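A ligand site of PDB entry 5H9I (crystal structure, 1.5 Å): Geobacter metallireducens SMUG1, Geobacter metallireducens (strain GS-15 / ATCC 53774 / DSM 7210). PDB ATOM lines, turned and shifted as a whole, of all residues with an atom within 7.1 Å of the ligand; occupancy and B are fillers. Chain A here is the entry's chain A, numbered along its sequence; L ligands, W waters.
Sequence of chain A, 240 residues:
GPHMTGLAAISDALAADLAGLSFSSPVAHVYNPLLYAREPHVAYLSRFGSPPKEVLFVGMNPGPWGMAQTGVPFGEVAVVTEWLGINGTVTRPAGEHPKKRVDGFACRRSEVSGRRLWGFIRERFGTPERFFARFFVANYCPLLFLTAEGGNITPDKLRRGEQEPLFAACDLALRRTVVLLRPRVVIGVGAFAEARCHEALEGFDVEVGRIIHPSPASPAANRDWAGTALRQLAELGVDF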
ATOM      1  N   VAL A  58      -2.749  14.151 -22.358  1.00  0.00           N
ATOM      2  CA  VAL A  58      -3.611  15.189 -21.889  1.00  0.00           C
ATOM      3  C   VAL A  58      -5.063  14.792 -22.106  1.00  0.00           C
ATOM      4  O   VAL A  58      -5.506  14.496 -23.217  1.00  0.00           O
ATOM      5  CB  VAL A  58      -3.379  16.524 -22.622  1.00  0.00           C
ATOM      6  CG1 VAL A  58      -4.257  17.617 -22.164  1.00  0.00           C
ATOM      7  CG2 VAL A  58      -1.919  16.835 -22.503  1.00  0.00           C
ATOM      8  N   GLY A  59      -5.797  14.643 -20.988  1.00  0.00           N
ATOM      9  CA  GLY A  59      -7.263  14.407 -21.050  1.00  0.00           C
ATOM     10  C   GLY A  59      -7.992  15.716 -21.106  1.00  0.00           C
ATOM     11  O   GLY A  59      -7.409  16.755 -21.092  1.00  0.00           O
ATOM     12  N   MET A  60      -9.269  15.622 -21.112  1.00  0.00           N
ATOM     13  CA  MET A  60     -10.124  16.793 -21.192  1.00  0.00           C
ATOM     14  C   MET A  60     -10.468  17.340 -19.834  1.00  0.00           C
ATOM     15  O   MET A  60     -10.079  18.396 -19.493  1.00  0.00           O
ATOM     16  CB  MET A  60     -11.394  16.435 -21.981  1.00  0.00           C
ATOM     17  CG  MET A  60     -12.448  17.565 -22.066  1.00  0.00           C
ATOM     18  SD  MET A  60     -13.980  17.089 -23.102  1.00  0.00           S
ATOM     19  CE  MET A  60     -14.668  16.012 -21.922  1.00  0.00           C
ATOM     20  N   ASN A  61     -11.246  16.602 -19.053  1.00  0.00           N
ATOM     21  CA  ASN A  61     -11.602  17.056 -17.741  1.00  0.00           C
ATOM     22  C   ASN A  61     -12.078  15.867 -16.889  1.00  0.00           C
ATOM     23  O   ASN A  61     -12.235  14.796 -17.428  1.00  0.00           O
ATOM     24  CB  ASN A  61     -12.644  18.235 -17.758  1.00  0.00           C
ATOM     25  CG  ASN A  61     -14.088  17.789 -17.942  1.00  0.00           C
ATOM     26  OD1 ASN A  61     -14.419  17.000 -18.834  1.00  0.00           O
ATOM     27  ND2 ASN A  61     -14.956  18.337 -17.093  1.00  0.00           N
ATOM     28  N   PRO A  62     -12.206  16.025 -15.569  1.00  0.00           N
ATOM     29  CA  PRO A  62     -12.502  14.860 -14.743  1.00  0.00           C
ATOM     30  C   PRO A  62     -13.788  14.138 -15.021  1.00  0.00           C
ATOM     31  O   PRO A  62     -14.784  14.767 -15.463  1.00  0.00           O
ATOM     32  CB  PRO A  62     -12.639  15.471 -13.356  1.00  0.00           C
ATOM     33  CG  PRO A  62     -11.680  16.671 -13.358  1.00  0.00           C
ATOM     34  CD  PRO A  62     -11.904  17.224 -14.755  1.00  0.00           C
ATOM     35  N   GLY A  63     -13.793  12.816 -14.834  1.00  0.00           N
ATOM     36  CA  GLY A  63     -15.074  12.109 -14.745  1.00  0.00           C
ATOM     37  C   GLY A  63     -15.457  12.163 -13.304  1.00  0.00           C
ATOM     38  O   GLY A  63     -14.663  12.238 -12.340  1.00  0.00           O
ATOM     39  N   PRO A  64     -16.780  12.139 -13.105  1.00  0.00           N
ATOM     40  CA  PRO A  64     -17.296  12.178 -11.723  1.00  0.00           C
ATOM     41  C   PRO A  64     -16.814  11.129 -10.777  1.00  0.00           C
ATOM     42  O   PRO A  64     -16.795  11.353  -9.539  1.00  0.00           O
ATOM     43  CB  PRO A  64     -18.852  12.047 -11.972  1.00  0.00           C
ATOM     44  CG  PRO A  64     -18.889  11.316 -13.261  1.00  0.00           C
ATOM     45  CD  PRO A  64     -17.834  11.979 -14.095  1.00  0.00           C
ATOM     46  N   GLY A  66     -13.841   9.426 -11.054  1.00  0.00           N
ATOM     47  CA  GLY A  66     -12.400   9.237 -11.165  1.00  0.00           C
ATOM     48  C   GLY A  66     -11.658  10.387 -10.525  1.00  0.00           C
ATOM     49  O   GLY A  66     -11.616  10.480  -9.311  1.00  0.00           O
ATOM     50  N   MET A  67     -11.193  11.312 -11.372  1.00  0.00           N
ATOM     51  CA  MET A  67     -10.405  12.457 -10.835  1.00  0.00           C
ATOM     52  C   MET A  67     -11.282  13.313  -9.833  1.00  0.00           C
ATOM     53  O   MET A  67     -10.756  13.884  -8.911  1.00  0.00           O
ATOM     54  CB  MET A  67      -9.835  13.344 -11.939  1.00  0.00           C
ATOM     55  CG  MET A  67      -9.106  14.471 -11.353  1.00  0.00           C
ATOM     56  SD  MET A  67      -8.026  15.261 -12.553  1.00  0.00           S
ATOM     57  CE  MET A  67      -7.378  16.671 -11.649  1.00  0.00           C
ATOM     58  N   ALA A  68     -12.612  13.348 -10.079  1.00  0.00           N
ATOM     59  CA  ALA A  68     -13.473  14.179  -9.141  1.00  0.00           C
ATOM     60  C   ALA A  68     -13.460  13.561  -7.805  1.00  0.00           C
ATOM     61  O   ALA A  68     -13.914  14.245  -6.835  1.00  0.00           O
ATOM     62  CB  ALA A  68     -14.844  14.301  -9.696  1.00  0.00           C
ATOM     63  N   VAL A  72      -6.678  12.468  -9.168  1.00  0.00           N
ATOM     64  CA  VAL A  72      -5.749  11.972 -10.130  1.00  0.00           C
ATOM     65  C   VAL A  72      -6.344  11.846 -11.469  1.00  0.00           C
ATOM     66  O   VAL A  72      -7.491  11.350 -11.544  1.00  0.00           O
ATOM     67  CB  VAL A  72      -5.230  10.647  -9.676  1.00  0.00           C
ATOM     68  CG1 VAL A  72      -4.320   9.995 -10.718  1.00  0.00           C
ATOM     69  CG2 VAL A  72      -4.485  10.766  -8.334  1.00  0.00           C
ATOM     70  N   PRO A  73      -5.768  12.359 -12.574  1.00  0.00           N
ATOM     71  CA  PRO A  73      -6.373  12.181 -13.916  1.00  0.00           C
ATOM     72  C   PRO A  73      -6.696  10.724 -14.227  1.00  0.00           C
ATOM     73  O   PRO A  73      -5.943   9.806 -13.911  1.00  0.00           O
ATOM     74  CB  PRO A  73      -5.301  12.713 -14.904  1.00  0.00           C
ATOM     75  CG  PRO A  73      -4.372  13.489 -14.031  1.00  0.00           C
ATOM     76  CD  PRO A  73      -4.440  12.970 -12.619  1.00  0.00           C
ATOM     77  N   PHE A  74      -7.905  10.557 -14.797  1.00  0.00           N
ATOM     78  CA  PHE A  74      -8.432   9.179 -15.082  1.00  0.00           C
ATOM     79  C   PHE A  74      -8.375   8.287 -13.867  1.00  0.00           C
ATOM     80  O   PHE A  74      -8.223   7.105 -13.943  1.00  0.00           O
ATOM     81  CB  PHE A  74      -7.637   8.561 -16.269  1.00  0.00           C
ATOM     82  CG  PHE A  74      -7.885   9.257 -17.600  1.00  0.00           C
ATOM     83  CD1 PHE A  74      -8.977   8.866 -18.409  1.00  0.00           C
ATOM     84  CD2 PHE A  74      -7.068  10.282 -18.018  1.00  0.00           C
ATOM     85  CE1 PHE A  74      -9.130   9.466 -19.624  1.00  0.00           C
ATOM     86  CE2 PHE A  74      -7.240  10.876 -19.224  1.00  0.00           C
ATOM     87  CZ  PHE A  74      -8.264  10.453 -20.004  1.00  0.00           C
ATOM     88  N   GLY A  75      -8.521   8.897 -12.664  1.00  0.00           N
ATOM     89  CA  GLY A  75      -8.128   8.282 -11.441  1.00  0.00           C
ATOM     90  C   GLY A  75      -9.186   7.401 -10.805  1.00  0.00           C
ATOM     91  O   GLY A  75      -9.715   7.724  -9.745  1.00  0.00           O
ATOM     92  N   GLU A 111     -14.698   3.922 -12.439  1.00  0.00           N
ATOM     93  CA  GLU A 111     -14.736   4.555 -13.715  1.00  0.00           C
ATOM     94  C   GLU A 111     -14.112   3.679 -14.798  1.00  0.00           C
ATOM     95  O   GLU A 111     -12.923   3.327 -14.661  1.00  0.00           O
ATOM     96  CB  GLU A 111     -13.961   5.896 -13.683  1.00  0.00           C
ATOM     97  CG  GLU A 111     -14.043   6.614 -15.014  1.00  0.00           C
ATOM     98  CD  GLU A 111     -13.069   7.776 -15.076  1.00  0.00           C
ATOM     99  OE1 GLU A 111     -12.038   7.717 -15.731  1.00  0.00           O
ATOM    100  OE2 GLU A 111     -13.405   8.846 -14.428  1.00  0.00           O
ATOM    101  N   VAL A 112     -14.857   3.363 -15.873  1.00  0.00           N
ATOM    102  CA  VAL A 112     -14.378   2.510 -16.900  1.00  0.00           C
ATOM    103  C   VAL A 112     -13.170   3.108 -17.626  1.00  0.00           C
ATOM    104  O   VAL A 112     -12.178   2.414 -17.913  1.00  0.00           O
ATOM    105  CB  VAL A 112     -15.480   2.107 -17.934  1.00  0.00           C
ATOM    106  CG1 VAL A 112     -14.991   1.183 -19.032  1.00  0.00           C
ATOM    107  CG2 VAL A 112     -16.603   1.392 -17.115  1.00  0.00           C
ATOM    108  N   SER A 113     -13.346   4.317 -18.001  1.00  0.00           N
ATOM    109  CA  SER A 113     -12.317   5.049 -18.770  1.00  0.00           C
ATOM    110  C   SER A 113     -10.966   4.986 -18.104  1.00  0.00           C
ATOM    111  O   SER A 113      -9.980   4.485 -18.700  1.00  0.00           O
ATOM    112  CB  SER A 113     -12.692   6.492 -19.012  1.00  0.00           C
ATOM    113  OG  SER A 113     -13.780   6.642 -19.885  1.00  0.00           O
ATOM    114  N   GLY A 114     -10.915   5.381 -16.863  1.00  0.00           N
ATOM    115  CA  GLY A 114      -9.603   5.361 -16.142  1.00  0.00           C
ATOM    116  C   GLY A 114      -9.135   3.992 -15.811  1.00  0.00           C
ATOM    117  O   GLY A 114      -7.951   3.614 -15.819  1.00  0.00           O
ATOM    118  N   VAL A 137       0.577  11.945 -17.257  1.00  0.00           N
ATOM    119  CA  VAL A 137      -0.825  12.140 -17.624  1.00  0.00           C
ATOM    120  C   VAL A 137      -1.406  13.314 -16.877  1.00  0.00           C
ATOM    121  O   VAL A 137      -1.300  13.386 -15.669  1.00  0.00           O
ATOM    122  CB  VAL A 137      -1.705  10.834 -17.332  1.00  0.00           C
ATOM    123  CG1 VAL A 137      -3.115  11.010 -17.768  1.00  0.00           C
ATOM    124  CG2 VAL A 137      -1.064   9.616 -18.011  1.00  0.00           C
ATOM    125  N   ALA A 138      -2.009  14.232 -17.587  1.00  0.00           N
ATOM    126  CA  ALA A 138      -2.630  15.404 -17.023  1.00  0.00           C
ATOM    127  C   ALA A 138      -3.937  15.721 -17.681  1.00  0.00           C
ATOM    128  O   ALA A 138      -4.202  15.204 -18.744  1.00  0.00           O
ATOM    129  CB  ALA A 138      -1.702  16.612 -17.204  1.00  0.00           C
ATOM    130  N   ASN A 139      -4.810  16.499 -17.010  1.00  0.00           N
ATOM    131  CA  ASN A 139      -6.015  16.975 -17.696  1.00  0.00           C
ATOM    132  C   ASN A 139      -5.802  18.418 -18.145  1.00  0.00           C
ATOM    133  O   ASN A 139      -5.246  19.197 -17.406  1.00  0.00           O
ATOM    134  CB  ASN A 139      -7.226  16.983 -16.774  1.00  0.00           C
ATOM    135  CG  ASN A 139      -8.030  15.746 -16.904  1.00  0.00           C
ATOM    136  OD1 ASN A 139      -8.037  15.073 -17.913  1.00  0.00           O
ATOM    137  ND2 ASN A 139      -8.593  15.313 -15.728  1.00  0.00           N
ATOM    138  N   TYR A 140      -6.400  18.770 -19.251  1.00  0.00           N
ATOM    139  CA  TYR A 140      -6.420  20.138 -19.717  1.00  0.00           C
ATOM    140  C   TYR A 140      -7.211  21.024 -18.754  1.00  0.00           C
ATOM    141  O   TYR A 140      -6.751  22.109 -18.425  1.00  0.00           O
ATOM    142  CB  TYR A 140      -7.090  20.122 -21.073  1.00  0.00           C
ATOM    143  CG  TYR A 140      -7.279  21.514 -21.686  1.00  0.00           C
ATOM    144  CD1 TYR A 140      -6.212  22.223 -22.097  1.00  0.00           C
ATOM    145  CD2 TYR A 140      -8.536  22.114 -21.685  1.00  0.00           C
ATOM    146  CE1 TYR A 140      -6.363  23.521 -22.607  1.00  0.00           C
ATOM    147  CE2 TYR A 140      -8.711  23.359 -22.170  1.00  0.00           C
ATOM    148  CZ  TYR A 140      -7.652  24.022 -22.664  1.00  0.00           C
ATOM    149  OH  TYR A 140      -7.839  25.311 -23.148  1.00  0.00           O
ATOM    150  N   CYS A 141      -8.396  20.536 -18.345  1.00  0.00           N
ATOM    151  CA  CYS A 141      -9.294  21.305 -17.464  1.00  0.00           C
ATOM    152  C   CYS A 141      -9.541  20.492 -16.232  1.00  0.00           C
ATOM    153  O   CYS A 141      -9.931  19.381 -16.325  1.00  0.00           O
ATOM    154  CB  CYS A 141     -10.564  21.610 -18.252  1.00  0.00           C
ATOM    155  SG  CYS A 141     -11.842  22.420 -17.239  1.00  0.00           S
ATOM    156  N   VAL A 189      -5.963  12.731 -25.339  1.00  0.00           N
ATOM    157  CA  VAL A 189      -6.818  11.527 -25.207  1.00  0.00           C
ATOM    158  C   VAL A 189      -8.223  12.001 -25.579  1.00  0.00           C
ATOM    159  O   VAL A 189      -8.924  12.677 -24.828  1.00  0.00           O
ATOM    160  CB  VAL A 189      -6.761  10.979 -23.819  1.00  0.00           C
ATOM    161  CG1 VAL A 189      -7.654   9.725 -23.703  1.00  0.00           C
ATOM    162  CG2 VAL A 189      -5.323  10.704 -23.397  1.00  0.00           C
ATOM    163  N   ALA A 193      -9.420  17.076 -26.360  1.00  0.00           N
ATOM    164  CA  ALA A 193      -8.104  17.321 -25.796  1.00  0.00           C
ATOM    165  C   ALA A 193      -7.099  17.524 -26.872  1.00  0.00           C
ATOM    166  O   ALA A 193      -6.282  18.409 -26.741  1.00  0.00           O
ATOM    167  CB  ALA A 193      -7.678  16.188 -24.849  1.00  0.00           C
ATOM    168  N   HIS A 213     -10.156   7.880 -27.194  1.00  0.00           N
ATOM    169  CA  HIS A 213     -10.561   7.958 -25.797  1.00  0.00           C
ATOM    170  C   HIS A 213     -11.109   6.619 -25.337  1.00  0.00           C
ATOM    171  O   HIS A 213     -11.796   5.923 -26.098  1.00  0.00           O
ATOM    172  CB  HIS A 213     -11.615   9.035 -25.679  1.00  0.00           C
ATOM    173  CG  HIS A 213     -11.900   9.413 -24.281  1.00  0.00           C
ATOM    174  ND1 HIS A 213     -12.614   8.594 -23.433  1.00  0.00           N
ATOM    175  CD2 HIS A 213     -11.540  10.492 -23.563  1.00  0.00           C
ATOM    176  CE1 HIS A 213     -12.703   9.178 -22.254  1.00  0.00           C
ATOM    177  NE2 HIS A 213     -12.106  10.334 -22.324  1.00  0.00           N
ATOM    178  N   PRO A 214     -10.812   6.217 -24.121  1.00  0.00           N
ATOM    179  CA  PRO A 214     -11.177   4.875 -23.626  1.00  0.00           C
ATOM    180  C   PRO A 214     -12.657   4.701 -23.228  1.00  0.00           C
ATOM    181  O   PRO A 214     -12.935   3.564 -22.857  1.00  0.00           O
ATOM    182  CB  PRO A 214     -10.209   4.673 -22.420  1.00  0.00           C
ATOM    183  CG  PRO A 214      -9.950   6.043 -21.906  1.00  0.00           C
ATOM    184  CD  PRO A 214      -9.836   6.866 -23.160  1.00  0.00           C
ATOM    185  N   SER A 215     -13.448   5.721 -23.252  1.00  0.00           N
ATOM    186  CA  SER A 215     -14.858   5.556 -22.782  1.00  0.00           C
ATOM    187  C   SER A 215     -15.649   4.593 -23.638  1.00  0.00           C
ATOM    188  O   SER A 215     -15.413   4.424 -24.860  1.00  0.00           O
ATOM    189  CB  SER A 215     -15.610   6.795 -22.479  1.00  0.00           C
ATOM    190  OG  SER A 215     -16.410   7.125 -23.495  1.00  0.00           O
HETATM  191  N1  LIG L   1     -12.371  10.023 -17.490  1.00  0.00           N
HETATM  192  C1  LIG L   1     -11.501  10.993 -17.436  1.00  0.00           C
HETATM  193  N2  LIG L   1     -10.645  11.426 -16.512  1.00  0.00           N
HETATM  194  C2  LIG L   1      -9.912  12.415 -16.757  1.00  0.00           C
HETATM  195  O1  LIG L   1      -9.178  12.815 -15.880  1.00  0.00           O
HETATM  196  N3  LIG L   1      -9.876  13.032 -17.945  1.00  0.00           N
HETATM  197  C3  LIG L   1     -10.640  12.693 -18.940  1.00  0.00           C
HETATM  198  O2  LIG L   1     -10.673  13.293 -20.021  1.00  0.00           O
HETATM  199  C4  LIG L   1     -11.543  11.649 -18.707  1.00  0.00           C
HETATM  200  N4  LIG L   1     -12.448  11.046 -19.464  1.00  0.00           N
HETATM  201  C5  LIG L   1     -12.947  10.066 -18.731  1.00  0.00           C
HETATM  202  O   HOH W   1     -11.732  10.946 -14.102  1.00  0.00           O
HETATM  203  O   HOH W   2     -12.963  13.509 -21.734  1.00  0.00           O
HETATM  204  O   HOH W   3     -14.570  13.612 -18.752  1.00  0.00           O
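Water W1 lies within hydrogen-bond range of N2 of the ligand (2.7 Å), OE2 of Glu 111 (2.7 Å), N of Met 67 (2.8 Å) and N of Gly 63 (2.9 Å).
Water W2 bridges O2 of the ligand (2.9 Å) and NE2 of His 213 (3.3 Å).
Water W3 lies within hydrogen-bond range of O of Asn 61, N4 of the ligand and O of Pro 62.
N4 of the ligand lies within hydrogen-bond range of NE2 of His 213 (3.0 Å).
The backbone carbonyl oxygen of Asn 61 lies within hydrogen-bond range of a nitrogen (N3) of the ligand.
The side-chain amide nitrogen of Asn 139 is in hydrogen-bond range of an oxygen (O1) of the ligand (2.6 Å).
The backbone NH (N) of Asn 61 is in hydrogen-bond range of an oxygen (O2) of the ligand (3.5 Å).
The backbone NH of Phe 74 is in hydrogen-bond range of an oxygen (O1) of the ligand, 2.8 Å away.
N of Met 60 sits at hydrogen-bond distance from O2 of the ligand.
A nitrogen (N1) of the ligand is in hydrogen-bond range of the side-chain carboxylate (OE1) of Glu 111 (2.9 Å).
Residues that only touch the ligand: Gly 59, Gly 63, Pro 73 and Ser 113.
Hydrophobic or aromatic side chains that line the ligand: Met 60, Pro 73, Phe 74 and His 213.
N of Gly 59 lies within hydrogen-bond range of O of Ala 138.
N of Ser 215 lies within hydrogen-bond range of ND1 of His 213, at 3.0 Å.
The side-chain sulfur of Met 67 is in hydrogen-bond range of the side-chain amide nitrogen of Asn 139 (3.2 Å).
The backbone carbonyl oxygen (O) of Gly 59 lies within hydrogen-bond range of the backbone NH (N) of Tyr 140 (2.9 Å).
The backbone NH (N) of Met 60 is in hydrogen-bond range of the side-chain amide oxygen (OD1) of Asn 139, at 3.5 Å.
The backbone NH (N) of Gly 114 sits at hydrogen-bond distance from the side-chain carboxylate (OE1) of Glu 111, at 2.8 Å.
O of Gly 63 sits at hydrogen-bond distance from N of Ala 68.
The backbone NH of Gly 66 lies close to the side-chain carboxylate of Glu 111 (3.5 Å).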
